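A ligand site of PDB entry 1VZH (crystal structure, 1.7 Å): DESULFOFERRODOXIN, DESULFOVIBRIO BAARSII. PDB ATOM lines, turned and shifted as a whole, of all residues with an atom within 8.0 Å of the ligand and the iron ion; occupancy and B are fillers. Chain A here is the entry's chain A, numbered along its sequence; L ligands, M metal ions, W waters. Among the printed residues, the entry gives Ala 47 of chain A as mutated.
The backbone NH (N) of Ala 45 sits at hydrogen-bond distance from a nitrogen (N5) of the ligand, 3.3 Å away.
The side-chain amino group (NZ) of Lys 48 lies within hydrogen-bond range of a nitrogen (N2) of the ligand (3.1 Å).
O of His 49 sits close to OE2 of Glu 114.
The backbone carbonyl oxygen (O) of His 119 is in hydrogen-bond range of the indole nitrogen (NE1) of Trp 122, 2.9 Å away.
The side-chain sulfur of Cys 116 lies close to the backbone NH of Ile 118 (3.5 Å).
O of Ala 45 sits at hydrogen-bond distance from ND1 of His 49, at 2.7 Å.
The backbone NH of His 69 is in hydrogen-bond range of the backbone carbonyl oxygen of Val 64, 2.9 Å away.
The backbone NH (N) of Cys 116 sits at hydrogen-bond distance from the side-chain carboxylate (OE1) of Glu 114, 3.3 Å away.
Residues that only touch the ligand: Pro 70 (3.7 Å) and Ala 44 (3.7 Å).
Hydrophobic or aromatic side chains within 4 Å of the ligand: Ala 44, Ala 45, His 49, His 69, Pro 70, His 75 and His 119.
Along chain A the residues within 4 Å of the ligand span positions 44 to 119.
The nearest printed residue that does not touch the ligand is Cys 116 (5.1 Å).
A ring nitrogen (ND1) of His 119 binds the iron ion.
The iron ion is bound by a ring nitrogen (NE2) of His 75 (2.2 Å).
NE2 of His 69 binds the iron ion.
The iron ion is bound by NE2 of His 49 (2.2 Å).
The iron ion is bound by N1 of the ligand (2.4 Å).
The side-chain sulfur (SG) of Cys 116 binds the iron ion (2.7 Å).
The iron ion has six donor atoms within binding distance.
Water W2 lies within hydrogen-bond range of a ring nitrogen (NE2) of His 119 (2.9 Å) and a nitrogen (N4) of the ligand (3.3 Å).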
ATOM      1  N   VAL A  42      -9.557   9.436 -12.737  1.00  0.00           N
ATOM      2  CA  VAL A  42     -10.780   8.641 -12.847  1.00  0.00           C
ATOM      3  C   VAL A  42     -12.040   9.496 -12.820  1.00  0.00           C
ATOM      4  O   VAL A  42     -12.144  10.461 -12.062  1.00  0.00           O
ATOM      5  CB  VAL A  42     -10.859   7.582 -11.727  1.00  0.00           C
ATOM      6  CG1 VAL A  42     -12.208   6.875 -11.763  1.00  0.00           C
ATOM      7  CG2 VAL A  42      -9.734   6.565 -11.895  1.00  0.00           C
ATOM      8  N   ASP A  43     -13.008   9.121 -13.657  1.00  0.00           N
ATOM      9  CA  ASP A  43     -14.279   9.828 -13.728  1.00  0.00           C
ATOM     10  C   ASP A  43     -15.170   9.399 -12.565  1.00  0.00           C
ATOM     11  O   ASP A  43     -16.035   8.542 -12.714  1.00  0.00           O
ATOM     12  CB  ASP A  43     -14.976   9.509 -15.055  1.00  0.00           C
ATOM     13  CG  ASP A  43     -16.229  10.339 -15.275  1.00  0.00           C
ATOM     14  OD1 ASP A  43     -17.146  10.283 -14.443  1.00  0.00           O
ATOM     15  OD2 ASP A  43     -16.287  11.047 -16.305  1.00  0.00           O
ATOM     16  N   ALA A  44     -14.944   9.990 -11.397  1.00  0.00           N
ATOM     17  CA  ALA A  44     -15.733   9.675 -10.201  1.00  0.00           C
ATOM     18  C   ALA A  44     -15.968  10.955  -9.405  1.00  0.00           C
ATOM     19  O   ALA A  44     -15.287  11.960  -9.621  1.00  0.00           O
ATOM     20  CB  ALA A  44     -15.004   8.635  -9.345  1.00  0.00           C
ATOM     21  N   ALA A  45     -16.924  10.909  -8.489  1.00  0.00           N
ATOM     22  CA  ALA A  45     -17.265  12.084  -7.675  1.00  0.00           C
ATOM     23  C   ALA A  45     -16.087  12.575  -6.840  1.00  0.00           C
ATOM     24  O   ALA A  45     -15.554  11.841  -6.006  1.00  0.00           O
ATOM     25  CB  ALA A  45     -18.446  11.764  -6.781  1.00  0.00           C
ATOM     26  N   LYS A  46     -15.695  13.818  -7.063  1.00  0.00           N
ATOM     27  CA  LYS A  46     -14.586  14.406  -6.325  1.00  0.00           C
ATOM     28  C   LYS A  46     -14.979  14.633  -4.861  1.00  0.00           C
ATOM     29  O   LYS A  46     -14.140  14.553  -3.977  1.00  0.00           O
ATOM     30  CB  LYS A  46     -14.168  15.740  -6.946  1.00  0.00           C
ATOM     31  CG  LYS A  46     -13.671  15.620  -8.381  1.00  0.00           C
ATOM     32  CD  LYS A  46     -13.182  16.960  -8.910  1.00  0.00           C
ATOM     33  CE  LYS A  46     -14.253  18.036  -8.805  1.00  0.00           C
ATOM     34  NZ  LYS A  46     -15.475  17.703  -9.589  1.00  0.00           N
ATOM     35  N   ALA A  47     -16.258  14.909  -4.635  1.00  0.00           N
ATOM     36  CA  ALA A  47     -16.762  15.150  -3.275  1.00  0.00           C
ATOM     37  C   ALA A  47     -16.440  14.012  -2.314  1.00  0.00           C
ATOM     38  O   ALA A  47     -16.163  14.241  -1.132  1.00  0.00           O
ATOM     39  CB  ALA A  47     -18.268  15.390  -3.314  1.00  0.00           C
ATOM     40  N   LYS A  48     -16.471  12.777  -2.819  1.00  0.00           N
ATOM     41  CA  LYS A  48     -16.182  11.628  -1.974  1.00  0.00           C
ATOM     42  C   LYS A  48     -14.767  11.069  -2.128  1.00  0.00           C
ATOM     43  O   LYS A  48     -14.342  10.261  -1.298  1.00  0.00           O
ATOM     44  CB  LYS A  48     -17.187  10.497  -2.238  1.00  0.00           C
ATOM     45  CG  LYS A  48     -18.607  10.799  -1.800  1.00  0.00           C
ATOM     46  CD  LYS A  48     -19.477   9.557  -1.881  1.00  0.00           C
ATOM     47  CE  LYS A  48     -20.906   9.834  -1.416  1.00  0.00           C
ATOM     48  NZ  LYS A  48     -21.741   8.611  -1.501  1.00  0.00           N
ATOM     49  N   HIS A  49     -14.046  11.488  -3.162  1.00  0.00           N
ATOM     50  CA  HIS A  49     -12.709  10.958  -3.391  1.00  0.00           C
ATOM     51  C   HIS A  49     -11.516  11.876  -3.169  1.00  0.00           C
ATOM     52  O   HIS A  49     -10.426  11.404  -2.850  1.00  0.00           O
ATOM     53  CB  HIS A  49     -12.610  10.379  -4.805  1.00  0.00           C
ATOM     54  CG  HIS A  49     -13.519   9.203  -5.027  1.00  0.00           C
ATOM     55  ND1 HIS A  49     -14.770   9.343  -5.588  1.00  0.00           N
ATOM     56  CD2 HIS A  49     -13.371   7.899  -4.744  1.00  0.00           C
ATOM     57  CE1 HIS A  49     -15.353   8.152  -5.641  1.00  0.00           C
ATOM     58  NE2 HIS A  49     -14.527   7.259  -5.129  1.00  0.00           N
ATOM     59  N   VAL A  64     -11.629  11.513   3.689  1.00  0.00           N
ATOM     60  CA  VAL A  64     -11.968  11.195   2.304  1.00  0.00           C
ATOM     61  C   VAL A  64     -13.478  11.012   2.194  1.00  0.00           C
ATOM     62  O   VAL A  64     -14.014   9.988   2.614  1.00  0.00           O
ATOM     63  CB  VAL A  64     -11.274   9.879   1.859  1.00  0.00           C
ATOM     64  CG1 VAL A  64     -11.651   9.543   0.423  1.00  0.00           C
ATOM     65  CG2 VAL A  64      -9.763  10.004   2.001  1.00  0.00           C
ATOM     66  N   VAL A  67     -17.315  14.732   1.380  1.00  0.00           N
ATOM     67  CA  VAL A  67     -18.461  13.931   1.769  1.00  0.00           C
ATOM     68  C   VAL A  67     -17.862  12.573   2.110  1.00  0.00           C
ATOM     69  O   VAL A  67     -17.105  12.018   1.320  1.00  0.00           O
ATOM     70  CB  VAL A  67     -19.465  13.773   0.601  1.00  0.00           C
ATOM     71  CG1 VAL A  67     -20.603  12.851   1.019  1.00  0.00           C
ATOM     72  CG2 VAL A  67     -20.006  15.131   0.185  1.00  0.00           C
ATOM     73  N   ALA A  68     -18.184  12.053   3.289  1.00  0.00           N
ATOM     74  CA  ALA A  68     -17.657  10.762   3.723  1.00  0.00           C
ATOM     75  C   ALA A  68     -17.819   9.660   2.686  1.00  0.00           C
ATOM     76  O   ALA A  68     -18.930   9.370   2.229  1.00  0.00           O
ATOM     77  CB  ALA A  68     -18.322  10.348   5.020  1.00  0.00           C
ATOM     78  N   HIS A  69     -16.701   9.036   2.301  1.00  0.00           N
ATOM     79  CA  HIS A  69     -16.711   7.961   1.315  1.00  0.00           C
ATOM     80  C   HIS A  69     -17.149   6.651   1.974  1.00  0.00           C
ATOM     81  O   HIS A  69     -16.879   6.412   3.159  1.00  0.00           O
ATOM     82  CB  HIS A  69     -15.314   7.799   0.703  1.00  0.00           C
ATOM     83  CG  HIS A  69     -15.236   6.777  -0.392  1.00  0.00           C
ATOM     84  ND1 HIS A  69     -15.209   5.422  -0.145  1.00  0.00           N
ATOM     85  CD2 HIS A  69     -15.153   6.919  -1.739  1.00  0.00           C
ATOM     86  CE1 HIS A  69     -15.127   4.767  -1.292  1.00  0.00           C
ATOM     87  NE2 HIS A  69     -15.086   5.650  -2.277  1.00  0.00           N
ATOM     88  N   PRO A  70     -17.835   5.784   1.217  1.00  0.00           N
ATOM     89  CA  PRO A  70     -18.294   4.499   1.758  1.00  0.00           C
ATOM     90  C   PRO A  70     -17.132   3.612   2.220  1.00  0.00           C
ATOM     91  O   PRO A  70     -16.031   3.688   1.672  1.00  0.00           O
ATOM     92  CB  PRO A  70     -19.031   3.872   0.584  1.00  0.00           C
ATOM     93  CG  PRO A  70     -19.543   5.059  -0.163  1.00  0.00           C
ATOM     94  CD  PRO A  70     -18.378   6.001  -0.134  1.00  0.00           C
ATOM     95  N   GLU A  72     -17.478   0.016   2.673  1.00  0.00           N
ATOM     96  CA  GLU A  72     -18.163  -1.267   2.562  1.00  0.00           C
ATOM     97  C   GLU A  72     -17.219  -2.347   2.060  1.00  0.00           C
ATOM     98  O   GLU A  72     -16.208  -2.058   1.420  1.00  0.00           O
ATOM     99  CB  GLU A  72     -19.335  -1.129   1.584  1.00  0.00           C
ATOM    100  CG  GLU A  72     -20.311  -0.019   1.929  1.00  0.00           C
ATOM    101  CD  GLU A  72     -21.451   0.094   0.920  1.00  0.00           C
ATOM    102  OE1 GLU A  72     -22.119  -0.930   0.679  1.00  0.00           O
ATOM    103  OE2 GLU A  72     -21.660   1.191   0.377  1.00  0.00           O
ATOM    104  N   HIS A  75     -16.589  -1.811  -1.547  1.00  0.00           N
ATOM    105  CA  HIS A  75     -16.286  -0.449  -1.976  1.00  0.00           C
ATOM    106  C   HIS A  75     -15.809   0.365  -0.781  1.00  0.00           C
ATOM    107  O   HIS A  75     -16.609   0.826   0.032  1.00  0.00           O
ATOM    108  CB  HIS A  75     -17.539   0.211  -2.562  1.00  0.00           C
ATOM    109  CG  HIS A  75     -17.302   1.582  -3.089  1.00  0.00           C
ATOM    110  ND1 HIS A  75     -18.317   2.497  -3.274  1.00  0.00           N
ATOM    111  CD2 HIS A  75     -16.162   2.208  -3.485  1.00  0.00           C
ATOM    112  CE1 HIS A  75     -17.811   3.621  -3.758  1.00  0.00           C
ATOM    113  NE2 HIS A  75     -16.507   3.468  -3.901  1.00  0.00           N
ATOM    114  N   TYR A  76     -14.491   0.549  -0.677  1.00  0.00           N
ATOM    115  CA  TYR A  76     -13.935   1.289   0.443  1.00  0.00           C
ATOM    116  C   TYR A  76     -12.592   1.915   0.104  1.00  0.00           C
ATOM    117  O   TYR A  76     -12.028   1.654  -0.959  1.00  0.00           O
ATOM    118  CB  TYR A  76     -13.744   0.353   1.645  1.00  0.00           C
ATOM    119  CG  TYR A  76     -12.731  -0.759   1.421  1.00  0.00           C
ATOM    120  CD1 TYR A  76     -13.005  -1.815   0.561  1.00  0.00           C
ATOM    121  CD2 TYR A  76     -11.507  -0.752   2.092  1.00  0.00           C
ATOM    122  CE1 TYR A  76     -12.074  -2.843   0.362  1.00  0.00           C
ATOM    123  CE2 TYR A  76     -10.574  -1.774   1.906  1.00  0.00           C
ATOM    124  CZ  TYR A  76     -10.867  -2.808   1.037  1.00  0.00           C
ATOM    125  OH  TYR A  76      -9.946  -3.823   0.857  1.00  0.00           O
ATOM    126  N   ILE A  77     -12.093   2.736   1.015  1.00  0.00           N
ATOM    127  CA  ILE A  77     -10.798   3.394   0.837  1.00  0.00           C
ATOM    128  C   ILE A  77      -9.794   2.426   1.442  1.00  0.00           C
ATOM    129  O   ILE A  77      -9.854   2.115   2.628  1.00  0.00           O
ATOM    130  CB  ILE A  77     -10.746   4.754   1.595  1.00  0.00           C
ATOM    131  CG1 ILE A  77     -11.890   5.646   1.129  1.00  0.00           C
ATOM    132  CG2 ILE A  77      -9.398   5.438   1.354  1.00  0.00           C
ATOM    133  CD1 ILE A  77     -11.943   5.853  -0.373  1.00  0.00           C
ATOM    134  N   GLU A 114      -5.229   8.999  -1.415  1.00  0.00           N
ATOM    135  CA  GLU A 114      -6.107   7.938  -0.954  1.00  0.00           C
ATOM    136  C   GLU A 114      -6.386   7.061  -2.148  1.00  0.00           C
ATOM    137  O   GLU A 114      -6.407   7.546  -3.286  1.00  0.00           O
ATOM    138  CB  GLU A 114      -7.422   8.513  -0.413  1.00  0.00           C
ATOM    139  CG  GLU A 114      -8.297   9.203  -1.467  1.00  0.00           C
ATOM    140  CD  GLU A 114      -9.299   8.277  -2.145  1.00  0.00           C
ATOM    141  OE1 GLU A 114      -9.206   7.044  -1.973  1.00  0.00           O
ATOM    142  OE2 GLU A 114     -10.181   8.795  -2.860  1.00  0.00           O
ATOM    143  N   TYR A 115      -6.569   5.776  -1.896  1.00  0.00           N
ATOM    144  CA  TYR A 115      -6.861   4.844  -2.972  1.00  0.00           C
ATOM    145  C   TYR A 115      -8.159   4.093  -2.684  1.00  0.00           C
ATOM    146  O   TYR A 115      -8.310   3.456  -1.649  1.00  0.00           O
ATOM    147  CB  TYR A 115      -5.712   3.848  -3.151  1.00  0.00           C
ATOM    148  CG  TYR A 115      -5.937   2.913  -4.317  1.00  0.00           C
ATOM    149  CD1 TYR A 115      -6.627   1.707  -4.151  1.00  0.00           C
ATOM    150  CD2 TYR A 115      -5.490   3.246  -5.596  1.00  0.00           C
ATOM    151  CE1 TYR A 115      -6.868   0.854  -5.236  1.00  0.00           C
ATOM    152  CE2 TYR A 115      -5.722   2.396  -6.683  1.00  0.00           C
ATOM    153  CZ  TYR A 115      -6.414   1.214  -6.496  1.00  0.00           C
ATOM    154  OH  TYR A 115      -6.674   0.398  -7.572  1.00  0.00           O
ATOM    155  N   CYS A 116      -9.106   4.219  -3.616  1.00  0.00           N
ATOM    156  CA  CYS A 116     -10.400   3.539  -3.514  1.00  0.00           C
ATOM    157  C   CYS A 116     -10.318   2.269  -4.370  1.00  0.00           C
ATOM    158  O   CYS A 116      -9.874   2.327  -5.530  1.00  0.00           O
ATOM    159  CB  CYS A 116     -11.500   4.455  -4.041  1.00  0.00           C
ATOM    160  SG  CYS A 116     -13.133   3.657  -4.188  1.00  0.00           S
ATOM    161  N   ASN A 117     -10.731   1.132  -3.820  1.00  0.00           N
ATOM    162  CA  ASN A 117     -10.636  -0.124  -4.552  1.00  0.00           C
ATOM    163  C   ASN A 117     -11.399  -0.090  -5.880  1.00  0.00           C
ATOM    164  O   ASN A 117     -11.082  -0.844  -6.805  1.00  0.00           O
ATOM    165  CB  ASN A 117     -11.141  -1.294  -3.684  1.00  0.00           C
ATOM    166  CG  ASN A 117     -12.643  -1.290  -3.512  1.00  0.00           C
ATOM    167  OD1 ASN A 117     -13.246  -0.286  -3.149  1.00  0.00           O
ATOM    168  ND2 ASN A 117     -13.265  -2.440  -3.749  1.00  0.00           N
ATOM    169  N   ILE A 118     -12.385   0.791  -5.976  1.00  0.00           N
ATOM    170  CA  ILE A 118     -13.160   0.911  -7.201  1.00  0.00           C
ATOM    171  C   ILE A 118     -12.787   2.115  -8.047  1.00  0.00           C
ATOM    172  O   ILE A 118     -12.578   1.987  -9.258  1.00  0.00           O
ATOM    173  CB  ILE A 118     -14.677   1.006  -6.889  1.00  0.00           C
ATOM    174  CG1 ILE A 118     -15.147  -0.265  -6.182  1.00  0.00           C
ATOM    175  CG2 ILE A 118     -15.470   1.210  -8.187  1.00  0.00           C
ATOM    176  CD1 ILE A 118     -14.916  -1.532  -6.984  1.00  0.00           C
ATOM    177  N   HIS A 119     -12.681   3.288  -7.423  1.00  0.00           N
ATOM    178  CA  HIS A 119     -12.396   4.509  -8.168  1.00  0.00           C
ATOM    179  C   HIS A 119     -10.982   5.037  -8.254  1.00  0.00           C
ATOM    180  O   HIS A 119     -10.768   6.200  -8.618  1.00  0.00           O
ATOM    181  CB  HIS A 119     -13.335   5.604  -7.673  1.00  0.00           C
ATOM    182  CG  HIS A 119     -14.782   5.226  -7.742  1.00  0.00           C
ATOM    183  ND1 HIS A 119     -15.527   4.920  -6.624  1.00  0.00           N
ATOM    184  CD2 HIS A 119     -15.593   5.025  -8.808  1.00  0.00           C
ATOM    185  CE1 HIS A 119     -16.742   4.548  -6.989  1.00  0.00           C
ATOM    186  NE2 HIS A 119     -16.810   4.606  -8.308  1.00  0.00           N
ATOM    187  N   GLY A 120     -10.007   4.207  -7.900  1.00  0.00           N
ATOM    188  CA  GLY A 120      -8.623   4.618  -8.032  1.00  0.00           C
ATOM    189  C   GLY A 120      -7.931   5.536  -7.035  1.00  0.00           C
ATOM    190  O   GLY A 120      -8.350   5.721  -5.891  1.00  0.00           O
ATOM    191  N   TRP A 122      -6.357   9.162  -5.737  1.00  0.00           N
ATOM    192  CA  TRP A 122      -6.689  10.580  -5.650  1.00  0.00           C
ATOM    193  C   TRP A 122      -5.749  11.324  -4.709  1.00  0.00           C
ATOM    194  O   TRP A 122      -5.203  10.729  -3.781  1.00  0.00           O
ATOM    195  CB  TRP A 122      -8.113  10.781  -5.160  1.00  0.00           C
ATOM    196  CG  TRP A 122      -9.119  10.187  -6.068  1.00  0.00           C
ATOM    197  CD1 TRP A 122      -9.418   8.865  -6.207  1.00  0.00           C
ATOM    198  CD2 TRP A 122      -9.933  10.896  -7.011  1.00  0.00           C
ATOM    199  NE1 TRP A 122     -10.369   8.708  -7.178  1.00  0.00           N
ATOM    200  CE2 TRP A 122     -10.703   9.934  -7.688  1.00  0.00           C
ATOM    201  CE3 TRP A 122     -10.073  12.246  -7.346  1.00  0.00           C
ATOM    202  CZ2 TRP A 122     -11.619  10.274  -8.694  1.00  0.00           C
ATOM    203  CZ3 TRP A 122     -10.981  12.599  -8.350  1.00  0.00           C
ATOM    204  CH2 TRP A 122     -11.739  11.608  -9.008  1.00  0.00           C
HETATM  205  N1  LIG L   1     -17.355   6.514  -4.257  1.00  0.00           N
HETATM  206  C1  LIG L   1     -18.362   6.744  -4.795  1.00  0.00           C
HETATM  207 FE1  LIG L   1     -20.031   7.124  -5.700  1.00  0.00          FE
HETATM  208  C2  LIG L   1     -20.930   6.428  -4.134  1.00  0.00           C
HETATM  209  N2  LIG L   1     -21.465   6.002  -3.185  1.00  0.00           N
HETATM  210  C3  LIG L   1     -20.149   8.946  -5.282  1.00  0.00           C
HETATM  211  N3  LIG L   1     -20.226  10.078  -5.017  1.00  0.00           N
HETATM  212  C4  LIG L   1     -19.966   5.311  -6.310  1.00  0.00           C
HETATM  213  N4  LIG L   1     -19.932   4.208  -6.684  1.00  0.00           N
HETATM  214  C5  LIG L   1     -19.098   7.690  -7.282  1.00  0.00           C
HETATM  215  N5  LIG L   1     -18.522   8.039  -8.240  1.00  0.00           N
HETATM  216  C6  LIG L   1     -21.701   7.360  -6.604  1.00  0.00           C
HETATM  217  N6  LIG L   1     -22.720   7.506  -7.159  1.00  0.00           N
HETATM  218 FE    FE M   1     -15.291   5.249  -4.475  1.00  0.00          FE
HETATM  219  O   HOH W   1     -21.019  12.786  -4.279  1.00  0.00           O
HETATM  220  O   HOH W   2     -19.127   3.765  -9.905  1.00  0.00           O
